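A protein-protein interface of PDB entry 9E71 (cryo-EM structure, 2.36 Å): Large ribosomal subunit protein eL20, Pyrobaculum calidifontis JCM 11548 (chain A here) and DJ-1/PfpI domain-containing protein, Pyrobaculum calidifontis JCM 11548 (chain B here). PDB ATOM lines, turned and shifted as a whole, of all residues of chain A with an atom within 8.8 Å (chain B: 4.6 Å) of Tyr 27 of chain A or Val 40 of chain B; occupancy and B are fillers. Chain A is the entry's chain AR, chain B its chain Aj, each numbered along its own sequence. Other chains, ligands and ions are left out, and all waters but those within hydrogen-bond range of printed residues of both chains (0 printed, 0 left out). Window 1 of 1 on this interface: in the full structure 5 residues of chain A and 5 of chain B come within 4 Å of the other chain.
Of the printed residues of chain B, Arg 25 of chain A touches Asn 41. Of chain B, only Arg 38, Val 40 and Asn 41 come within 4 Å of Tyr 27 of chain A. Of the printed residues of chain B, Leu 30 of chain A touches Arg 38. Lys 32 of chain A touches none of the printed residues of chain B. Thr 11 of chain B touches none of the printed residues of chain A. Printed residues of chain A within 4 Å of Arg 38 of chain B: Tyr 27 (3.5 Å) and Leu 30 (3.4 Å). No residue of chain A comes within 4 Å of Asp 39 of chain B. Of chain A, only Tyr 27 (3.6 Å) comes within 4 Å of Val 40 of chain B. The nearest residue of chain B that does not touch Tyr 27 of chain A is Asp 39 of chain B (4.1 Å).
Among the printed residues, merely in contact across the chains: Tyr 27 of chain A with Asn 41 of chain B, Leu 30 of chain A with Arg 38 of chain B, Tyr 27 of chain A with Arg 38 of chain B, Tyr 27 of chain A with Val 40 of chain B and Arg 25 of chain A with Asn 41 of chain B.
NH1 of Arg 25 of chain A lies within salt-bridge range of OD2 of Asp 28 of chain A (2.5 Å).
Of the 10 printed residues of chain B, 3 touch a printed residue of chain A. Printed residues of chain A that touch a printed residue of chain B: Arg 25, Tyr 27 and Leu 30. Hydrophobic or aromatic side chains of chain A that line the printed part of chain B: Tyr 27 and Leu 30.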
ATOM      1  N   TYR A   5     -28.125  -1.204 -12.411  1.00  0.00           N
ATOM      2  CA  TYR A   5     -27.095  -0.218 -12.687  1.00  0.00           C
ATOM      3  C   TYR A   5     -27.739   1.042 -13.238  1.00  0.00           C
ATOM      4  O   TYR A   5     -28.520   0.977 -14.192  1.00  0.00           O
ATOM      5  CB  TYR A   5     -26.069  -0.756 -13.683  1.00  0.00           C
ATOM      6  CG  TYR A   5     -25.161  -1.804 -13.104  1.00  0.00           C
ATOM      7  CD1 TYR A   5     -23.990  -1.449 -12.458  1.00  0.00           C
ATOM      8  CD2 TYR A   5     -25.477  -3.148 -13.197  1.00  0.00           C
ATOM      9  CE1 TYR A   5     -23.162  -2.399 -11.926  1.00  0.00           C
ATOM     10  CE2 TYR A   5     -24.651  -4.107 -12.663  1.00  0.00           C
ATOM     11  CZ  TYR A   5     -23.495  -3.725 -12.027  1.00  0.00           C
ATOM     12  OH  TYR A   5     -22.663  -4.673 -11.492  1.00  0.00           O
ATOM     13  N   VAL A   7     -27.035   4.214 -15.305  1.00  0.00           N
ATOM     14  CA  VAL A   7     -26.105   4.667 -16.330  1.00  0.00           C
ATOM     15  C   VAL A   7     -26.501   6.084 -16.709  1.00  0.00           C
ATOM     16  O   VAL A   7     -27.648   6.335 -17.094  1.00  0.00           O
ATOM     17  CB  VAL A   7     -26.122   3.745 -17.556  1.00  0.00           C
ATOM     18  CG1 VAL A   7     -25.018   4.129 -18.517  1.00  0.00           C
ATOM     19  CG2 VAL A   7     -25.986   2.302 -17.128  1.00  0.00           C
ATOM     20  N   VAL A  21     -30.537  -0.452 -15.759  1.00  0.00           N
ATOM     21  CA  VAL A  21     -30.395  -1.715 -16.472  1.00  0.00           C
ATOM     22  C   VAL A  21     -30.042  -2.814 -15.482  1.00  0.00           C
ATOM     23  O   VAL A  21     -29.117  -2.657 -14.680  1.00  0.00           O
ATOM     24  CB  VAL A  21     -29.328  -1.626 -17.577  1.00  0.00           C
ATOM     25  CG1 VAL A  21     -29.042  -2.997 -18.138  1.00  0.00           C
ATOM     26  CG2 VAL A  21     -29.793  -0.694 -18.672  1.00  0.00           C
ATOM     27  N   GLY A  23     -28.207  -6.012 -14.807  1.00  0.00           N
ATOM     28  CA  GLY A  23     -27.080  -6.697 -15.403  1.00  0.00           C
ATOM     29  C   GLY A  23     -26.208  -7.312 -14.334  1.00  0.00           C
ATOM     30  O   GLY A  23     -26.073  -6.790 -13.223  1.00  0.00           O
ATOM     31  N   GLU A  24     -25.610  -8.438 -14.696  1.00  0.00           N
ATOM     32  CA  GLU A  24     -24.711  -9.152 -13.800  1.00  0.00           C
ATOM     33  C   GLU A  24     -23.349  -8.474 -13.705  1.00  0.00           C
ATOM     34  O   GLU A  24     -22.551  -8.823 -12.828  1.00  0.00           O
ATOM     35  CB  GLU A  24     -24.571 -10.623 -14.234  1.00  0.00           C
ATOM     36  CG  GLU A  24     -23.886 -10.914 -15.583  1.00  0.00           C
ATOM     37  CD  GLU A  24     -24.732 -10.503 -16.775  1.00  0.00           C
ATOM     38  OE1 GLU A  24     -24.824  -9.283 -17.011  1.00  0.00           O
ATOM     39  OE2 GLU A  24     -25.345 -11.369 -17.428  1.00  0.00           O
ATOM     40  N   ARG A  25     -23.058  -7.521 -14.582  1.00  0.00           N
ATOM     41  CA  ARG A  25     -21.883  -6.681 -14.410  1.00  0.00           C
ATOM     42  C   ARG A  25     -22.057  -5.401 -15.209  1.00  0.00           C
ATOM     43  O   ARG A  25     -22.932  -5.310 -16.086  1.00  0.00           O
ATOM     44  CB  ARG A  25     -20.599  -7.402 -14.827  1.00  0.00           C
ATOM     45  CG  ARG A  25     -20.762  -8.432 -15.908  1.00  0.00           C
ATOM     46  CD  ARG A  25     -19.426  -9.084 -16.191  1.00  0.00           C
ATOM     47  NE  ARG A  25     -19.570 -10.478 -16.581  1.00  0.00           N
ATOM     48  CZ  ARG A  25     -19.734 -10.893 -17.827  1.00  0.00           C
ATOM     49  NH1 ARG A  25     -19.727 -10.047 -18.843  1.00  0.00           N
ATOM     50  NH2 ARG A  25     -19.908 -12.189 -18.062  1.00  0.00           N
ATOM     51  N   PRO A  26     -21.240  -4.383 -14.920  1.00  0.00           N
ATOM     52  CA  PRO A  26     -21.309  -3.125 -15.681  1.00  0.00           C
ATOM     53  C   PRO A  26     -21.050  -3.288 -17.169  1.00  0.00           C
ATOM     54  O   PRO A  26     -21.605  -2.523 -17.965  1.00  0.00           O
ATOM     55  CB  PRO A  26     -20.225  -2.266 -15.019  1.00  0.00           C
ATOM     56  CG  PRO A  26     -20.044  -2.837 -13.673  1.00  0.00           C
ATOM     57  CD  PRO A  26     -20.302  -4.297 -13.791  1.00  0.00           C
ATOM     58  N   TYR A  27     -20.223  -4.258 -17.565  1.00  0.00           N
ATOM     59  CA  TYR A  27     -19.963  -4.477 -18.983  1.00  0.00           C
ATOM     60  C   TYR A  27     -21.232  -4.887 -19.717  1.00  0.00           C
ATOM     61  O   TYR A  27     -21.536  -4.371 -20.798  1.00  0.00           O
ATOM     62  CB  TYR A  27     -18.875  -5.534 -19.162  1.00  0.00           C
ATOM     63  CG  TYR A  27     -18.708  -5.983 -20.594  1.00  0.00           C
ATOM     64  CD1 TYR A  27     -18.041  -5.187 -21.506  1.00  0.00           C
ATOM     65  CD2 TYR A  27     -19.212  -7.200 -21.031  1.00  0.00           C
ATOM     66  CE1 TYR A  27     -17.888  -5.579 -22.813  1.00  0.00           C
ATOM     67  CE2 TYR A  27     -19.065  -7.600 -22.340  1.00  0.00           C
ATOM     68  CZ  TYR A  27     -18.403  -6.785 -23.226  1.00  0.00           C
ATOM     69  OH  TYR A  27     -18.243  -7.183 -24.533  1.00  0.00           O
ATOM     70  N   ASP A  28     -22.001  -5.803 -19.135  1.00  0.00           N
ATOM     71  CA  ASP A  28     -23.238  -6.220 -19.780  1.00  0.00           C
ATOM     72  C   ASP A  28     -24.314  -5.153 -19.687  1.00  0.00           C
ATOM     73  O   ASP A  28     -25.150  -5.037 -20.594  1.00  0.00           O
ATOM     74  CB  ASP A  28     -23.729  -7.524 -19.182  1.00  0.00           C
ATOM     75  CG  ASP A  28     -22.804  -8.654 -19.483  1.00  0.00           C
ATOM     76  OD1 ASP A  28     -22.921  -9.191 -20.594  1.00  0.00           O
ATOM     77  OD2 ASP A  28     -21.969  -9.001 -18.626  1.00  0.00           O
ATOM     78  N   ALA A  29     -24.319  -4.371 -18.604  1.00  0.00           N
ATOM     79  CA  ALA A  29     -25.222  -3.225 -18.552  1.00  0.00           C
ATOM     80  C   ALA A  29     -24.920  -2.244 -19.678  1.00  0.00           C
ATOM     81  O   ALA A  29     -25.837  -1.736 -20.338  1.00  0.00           O
ATOM     82  CB  ALA A  29     -25.114  -2.531 -17.198  1.00  0.00           C
ATOM     83  N   LEU A  30     -23.636  -2.003 -19.943  1.00  0.00           N
ATOM     84  CA  LEU A  30     -23.255  -1.080 -21.003  1.00  0.00           C
ATOM     85  C   LEU A  30     -23.552  -1.655 -22.380  1.00  0.00           C
ATOM     86  O   LEU A  30     -23.912  -0.914 -23.298  1.00  0.00           O
ATOM     87  CB  LEU A  30     -21.777  -0.725 -20.867  1.00  0.00           C
ATOM     88  CG  LEU A  30     -21.523   0.143 -19.634  1.00  0.00           C
ATOM     89  CD1 LEU A  30     -20.047   0.319 -19.370  1.00  0.00           C
ATOM     90  CD2 LEU A  30     -22.206   1.488 -19.791  1.00  0.00           C
ATOM     91  N   GLU A  31     -23.392  -2.969 -22.545  1.00  0.00           N
ATOM     92  CA  GLU A  31     -23.730  -3.614 -23.809  1.00  0.00           C
ATOM     93  C   GLU A  31     -25.224  -3.466 -24.083  1.00  0.00           C
ATOM     94  O   GLU A  31     -25.630  -3.098 -25.194  1.00  0.00           O
ATOM     95  CB  GLU A  31     -23.315  -5.086 -23.732  1.00  0.00           C
ATOM     96  CG  GLU A  31     -23.489  -6.030 -24.931  1.00  0.00           C
ATOM     97  CD  GLU A  31     -23.339  -5.388 -26.310  1.00  0.00           C
ATOM     98  OE1 GLU A  31     -22.348  -5.719 -26.993  1.00  0.00           O
ATOM     99  OE2 GLU A  31     -24.226  -4.657 -26.777  1.00  0.00           O
ATOM    100  N   LYS A  32     -26.047  -3.676 -23.051  1.00  0.00           N
ATOM    101  CA  LYS A  32     -27.491  -3.482 -23.182  1.00  0.00           C
ATOM    102  C   LYS A  32     -27.829  -2.039 -23.540  1.00  0.00           C
ATOM    103  O   LYS A  32     -28.670  -1.786 -24.410  1.00  0.00           O
ATOM    104  CB  LYS A  32     -28.189  -3.887 -21.886  1.00  0.00           C
ATOM    105  CG  LYS A  32     -29.593  -4.413 -22.079  1.00  0.00           C
ATOM    106  CD  LYS A  32     -30.024  -5.275 -20.908  1.00  0.00           C
ATOM    107  CE  LYS A  32     -28.848  -6.040 -20.341  1.00  0.00           C
ATOM    108  NZ  LYS A  32     -29.279  -7.158 -19.464  1.00  0.00           N
ATOM    109  N   VAL A  33     -27.158  -1.081 -22.895  1.00  0.00           N
ATOM    110  CA  VAL A  33     -27.417   0.333 -23.168  1.00  0.00           C
ATOM    111  C   VAL A  33     -27.039   0.689 -24.603  1.00  0.00           C
ATOM    112  O   VAL A  33     -27.784   1.385 -25.300  1.00  0.00           O
ATOM    113  CB  VAL A  33     -26.670   1.220 -22.159  1.00  0.00           C
ATOM    114  CG1 VAL A  33     -26.800   2.675 -22.551  1.00  0.00           C
ATOM    115  CG2 VAL A  33     -27.202   0.992 -20.764  1.00  0.00           C
ATOM    116  N   TYR A  34     -25.878   0.215 -25.063  1.00  0.00           N
ATOM    117  CA  TYR A  34     -25.416   0.519 -26.416  1.00  0.00           C
ATOM    118  C   TYR A  34     -26.358  -0.049 -27.464  1.00  0.00           C
ATOM    119  O   TYR A  34     -26.763   0.656 -28.396  1.00  0.00           O
ATOM    120  CB  TYR A  34     -24.010  -0.033 -26.639  1.00  0.00           C
ATOM    121  CG  TYR A  34     -22.919   0.738 -25.948  1.00  0.00           C
ATOM    122  CD1 TYR A  34     -23.011   2.109 -25.779  1.00  0.00           C
ATOM    123  CD2 TYR A  34     -21.796   0.092 -25.461  1.00  0.00           C
ATOM    124  CE1 TYR A  34     -22.013   2.814 -25.146  1.00  0.00           C
ATOM    125  CE2 TYR A  34     -20.796   0.787 -24.826  1.00  0.00           C
ATOM    126  CZ  TYR A  34     -20.909   2.148 -24.671  1.00  0.00           C
ATOM    127  OH  TYR A  34     -19.910   2.848 -24.037  1.00  0.00           O
ATOM    128  N   ARG A  45     -22.010   3.756 -31.657  1.00  0.00           N
ATOM    129  CA  ARG A  45     -21.430   3.672 -30.322  1.00  0.00           C
ATOM    130  C   ARG A  45     -20.507   4.846 -30.032  1.00  0.00           C
ATOM    131  O   ARG A  45     -20.333   5.225 -28.869  1.00  0.00           O
ATOM    132  CB  ARG A  45     -20.685   2.349 -30.160  1.00  0.00           C
ATOM    133  CG  ARG A  45     -21.509   1.286 -29.478  1.00  0.00           C
ATOM    134  CD  ARG A  45     -21.114  -0.100 -29.916  1.00  0.00           C
ATOM    135  NE  ARG A  45     -22.253  -1.005 -29.872  1.00  0.00           N
ATOM    136  CZ  ARG A  45     -22.322  -2.086 -29.110  1.00  0.00           C
ATOM    137  NH1 ARG A  45     -21.323  -2.438 -28.321  1.00  0.00           N
ATOM    138  NH2 ARG A  45     -23.422  -2.830 -29.141  1.00  0.00           N
ATOM    139  N   VAL A  53     -21.528   5.071 -14.232  1.00  0.00           N
ATOM    140  CA  VAL A  53     -22.179   3.785 -14.012  1.00  0.00           C
ATOM    141  C   VAL A  53     -22.107   3.471 -12.526  1.00  0.00           C
ATOM    142  O   VAL A  53     -21.014   3.440 -11.950  1.00  0.00           O
ATOM    143  CB  VAL A  53     -21.525   2.664 -14.837  1.00  0.00           C
ATOM    144  CG1 VAL A  53     -22.176   1.335 -14.517  1.00  0.00           C
ATOM    145  CG2 VAL A  53     -21.628   2.974 -16.314  1.00  0.00           C
ATOM    146  N   VAL B   8      -6.685  -8.342 -15.479  1.00  0.00           N
ATOM    147  CA  VAL B   8      -6.966  -8.284 -16.914  1.00  0.00           C
ATOM    148  C   VAL B   8      -7.275  -6.824 -17.229  1.00  0.00           C
ATOM    149  O   VAL B   8      -8.422  -6.385 -17.194  1.00  0.00           O
ATOM    150  CB  VAL B   8      -8.103  -9.217 -17.318  1.00  0.00           C
ATOM    151  CG1 VAL B   8      -8.192  -9.313 -18.832  1.00  0.00           C
ATOM    152  CG2 VAL B   8      -7.910 -10.588 -16.709  1.00  0.00           C
ATOM    153  N   ILE B   9      -6.227  -6.058 -17.522  1.00  0.00           N
ATOM    154  CA  ILE B   9      -6.409  -4.643 -17.818  1.00  0.00           C
ATOM    155  C   ILE B   9      -7.064  -4.447 -19.177  1.00  0.00           C
ATOM    156  O   ILE B   9      -7.910  -3.563 -19.347  1.00  0.00           O
ATOM    157  CB  ILE B   9      -5.067  -3.903 -17.722  1.00  0.00           C
ATOM    158  CG1 ILE B   9      -4.465  -4.091 -16.332  1.00  0.00           C
ATOM    159  CG2 ILE B   9      -5.266  -2.434 -18.012  1.00  0.00           C
ATOM    160  CD1 ILE B   9      -2.963  -4.068 -16.305  1.00  0.00           C
ATOM    161  N   THR B  11      -8.469  -6.565 -22.951  1.00  0.00           N
ATOM    162  CA  THR B  11      -8.708  -7.736 -23.781  1.00  0.00           C
ATOM    163  C   THR B  11      -8.444  -7.461 -25.255  1.00  0.00           C
ATOM    164  O   THR B  11      -8.889  -8.234 -26.108  1.00  0.00           O
ATOM    165  CB  THR B  11     -10.139  -8.243 -23.596  1.00  0.00           C
ATOM    166  OG1 THR B  11     -11.018  -7.131 -23.396  1.00  0.00           O
ATOM    167  CG2 THR B  11     -10.221  -9.174 -22.404  1.00  0.00           C
ATOM    168  N   VAL B  35     -10.484  -7.182 -12.412  1.00  0.00           N
ATOM    169  CA  VAL B  35     -10.786  -6.245 -13.487  1.00  0.00           C
ATOM    170  C   VAL B  35     -10.991  -4.864 -12.886  1.00  0.00           C
ATOM    171  O   VAL B  35     -11.640  -4.719 -11.846  1.00  0.00           O
ATOM    172  CB  VAL B  35     -12.021  -6.702 -14.291  1.00  0.00           C
ATOM    173  CG1 VAL B  35     -12.647  -5.541 -15.028  1.00  0.00           C
ATOM    174  CG2 VAL B  35     -11.631  -7.797 -15.258  1.00  0.00           C
ATOM    175  N   SER B  37     -11.877  -2.062 -15.045  1.00  0.00           N
ATOM    176  CA  SER B  37     -12.525  -1.228 -16.044  1.00  0.00           C
ATOM    177  C   SER B  37     -13.802  -1.911 -16.507  1.00  0.00           C
ATOM    178  O   SER B  37     -13.963  -3.125 -16.371  1.00  0.00           O
ATOM    179  CB  SER B  37     -11.603  -0.950 -17.238  1.00  0.00           C
ATOM    180  OG  SER B  37     -11.538  -2.064 -18.107  1.00  0.00           O
ATOM    181  N   ARG B  38     -14.711  -1.111 -17.061  1.00  0.00           N
ATOM    182  CA  ARG B  38     -16.000  -1.617 -17.514  1.00  0.00           C
ATOM    183  C   ARG B  38     -15.969  -2.141 -18.942  1.00  0.00           C
ATOM    184  O   ARG B  38     -16.990  -2.641 -19.421  1.00  0.00           O
ATOM    185  CB  ARG B  38     -17.064  -0.524 -17.401  1.00  0.00           C
ATOM    186  CG  ARG B  38     -16.944   0.331 -16.158  1.00  0.00           C
ATOM    187  CD  ARG B  38     -17.703   1.636 -16.310  1.00  0.00           C
ATOM    188  NE  ARG B  38     -17.670   2.134 -17.680  1.00  0.00           N
ATOM    189  CZ  ARG B  38     -17.527   3.411 -18.009  1.00  0.00           C
ATOM    190  NH1 ARG B  38     -17.384   4.350 -17.089  1.00  0.00           N
ATOM    191  NH2 ARG B  38     -17.530   3.755 -19.294  1.00  0.00           N
ATOM    192  N   ASP B  39     -14.841  -2.037 -19.632  1.00  0.00           N
ATOM    193  CA  ASP B  39     -14.753  -2.462 -21.021  1.00  0.00           C
ATOM    194  C   ASP B  39     -14.208  -3.874 -21.187  1.00  0.00           C
ATOM    195  O   ASP B  39     -14.009  -4.311 -22.323  1.00  0.00           O
ATOM    196  CB  ASP B  39     -13.885  -1.484 -21.813  1.00  0.00           C
ATOM    197  CG  ASP B  39     -12.410  -1.766 -21.661  1.00  0.00           C
ATOM    198  OD1 ASP B  39     -11.917  -1.742 -20.516  1.00  0.00           O
ATOM    199  OD2 ASP B  39     -11.742  -2.016 -22.684  1.00  0.00           O
ATOM    200  N   VAL B  40     -13.959  -4.591 -20.100  1.00  0.00           N
ATOM    201  CA  VAL B  40     -13.449  -5.953 -20.171  1.00  0.00           C
ATOM    202  C   VAL B  40     -14.624  -6.919 -20.109  1.00  0.00           C
ATOM    203  O   VAL B  40     -15.503  -6.790 -19.249  1.00  0.00           O
ATOM    204  CB  VAL B  40     -12.446  -6.223 -19.040  1.00  0.00           C
ATOM    205  CG1 VAL B  40     -12.050  -7.682 -19.027  1.00  0.00           C
ATOM    206  CG2 VAL B  40     -11.226  -5.343 -19.207  1.00  0.00           C
ATOM    207  N   ASN B  41     -14.644  -7.885 -21.024  1.00  0.00           N
ATOM    208  CA  ASN B  41     -15.780  -8.779 -21.199  1.00  0.00           C
ATOM    209  C   ASN B  41     -15.638 -10.110 -20.474  1.00  0.00           C
ATOM    210  O   ASN B  41     -16.559 -10.928 -20.537  1.00  0.00           O
ATOM    211  CB  ASN B  41     -16.006  -9.043 -22.687  1.00  0.00           C
ATOM    212  CG  ASN B  41     -15.039 -10.051 -23.249  1.00  0.00           C
ATOM    213  OD1 ASN B  41     -13.829  -9.843 -23.227  1.00  0.00           O
ATOM    214  ND2 ASN B  41     -15.567 -11.150 -23.765  1.00  0.00           N
ATOM    215  N   VAL B  42     -14.532 -10.353 -19.803  1.00  0.00           N
ATOM    216  CA  VAL B  42     -14.299 -11.650 -19.180  1.00  0.00           C
ATOM    217  C   VAL B  42     -14.886 -11.647 -17.780  1.00  0.00           C
ATOM    218  O   VAL B  42     -14.958 -10.611 -17.112  1.00  0.00           O
ATOM    219  CB  VAL B  42     -12.799 -12.004 -19.154  1.00  0.00           C
ATOM    220  CG1 VAL B  42     -12.186 -11.824 -20.527  1.00  0.00           C
ATOM    221  CG2 VAL B  42     -12.076 -11.164 -18.122  1.00  0.00           C
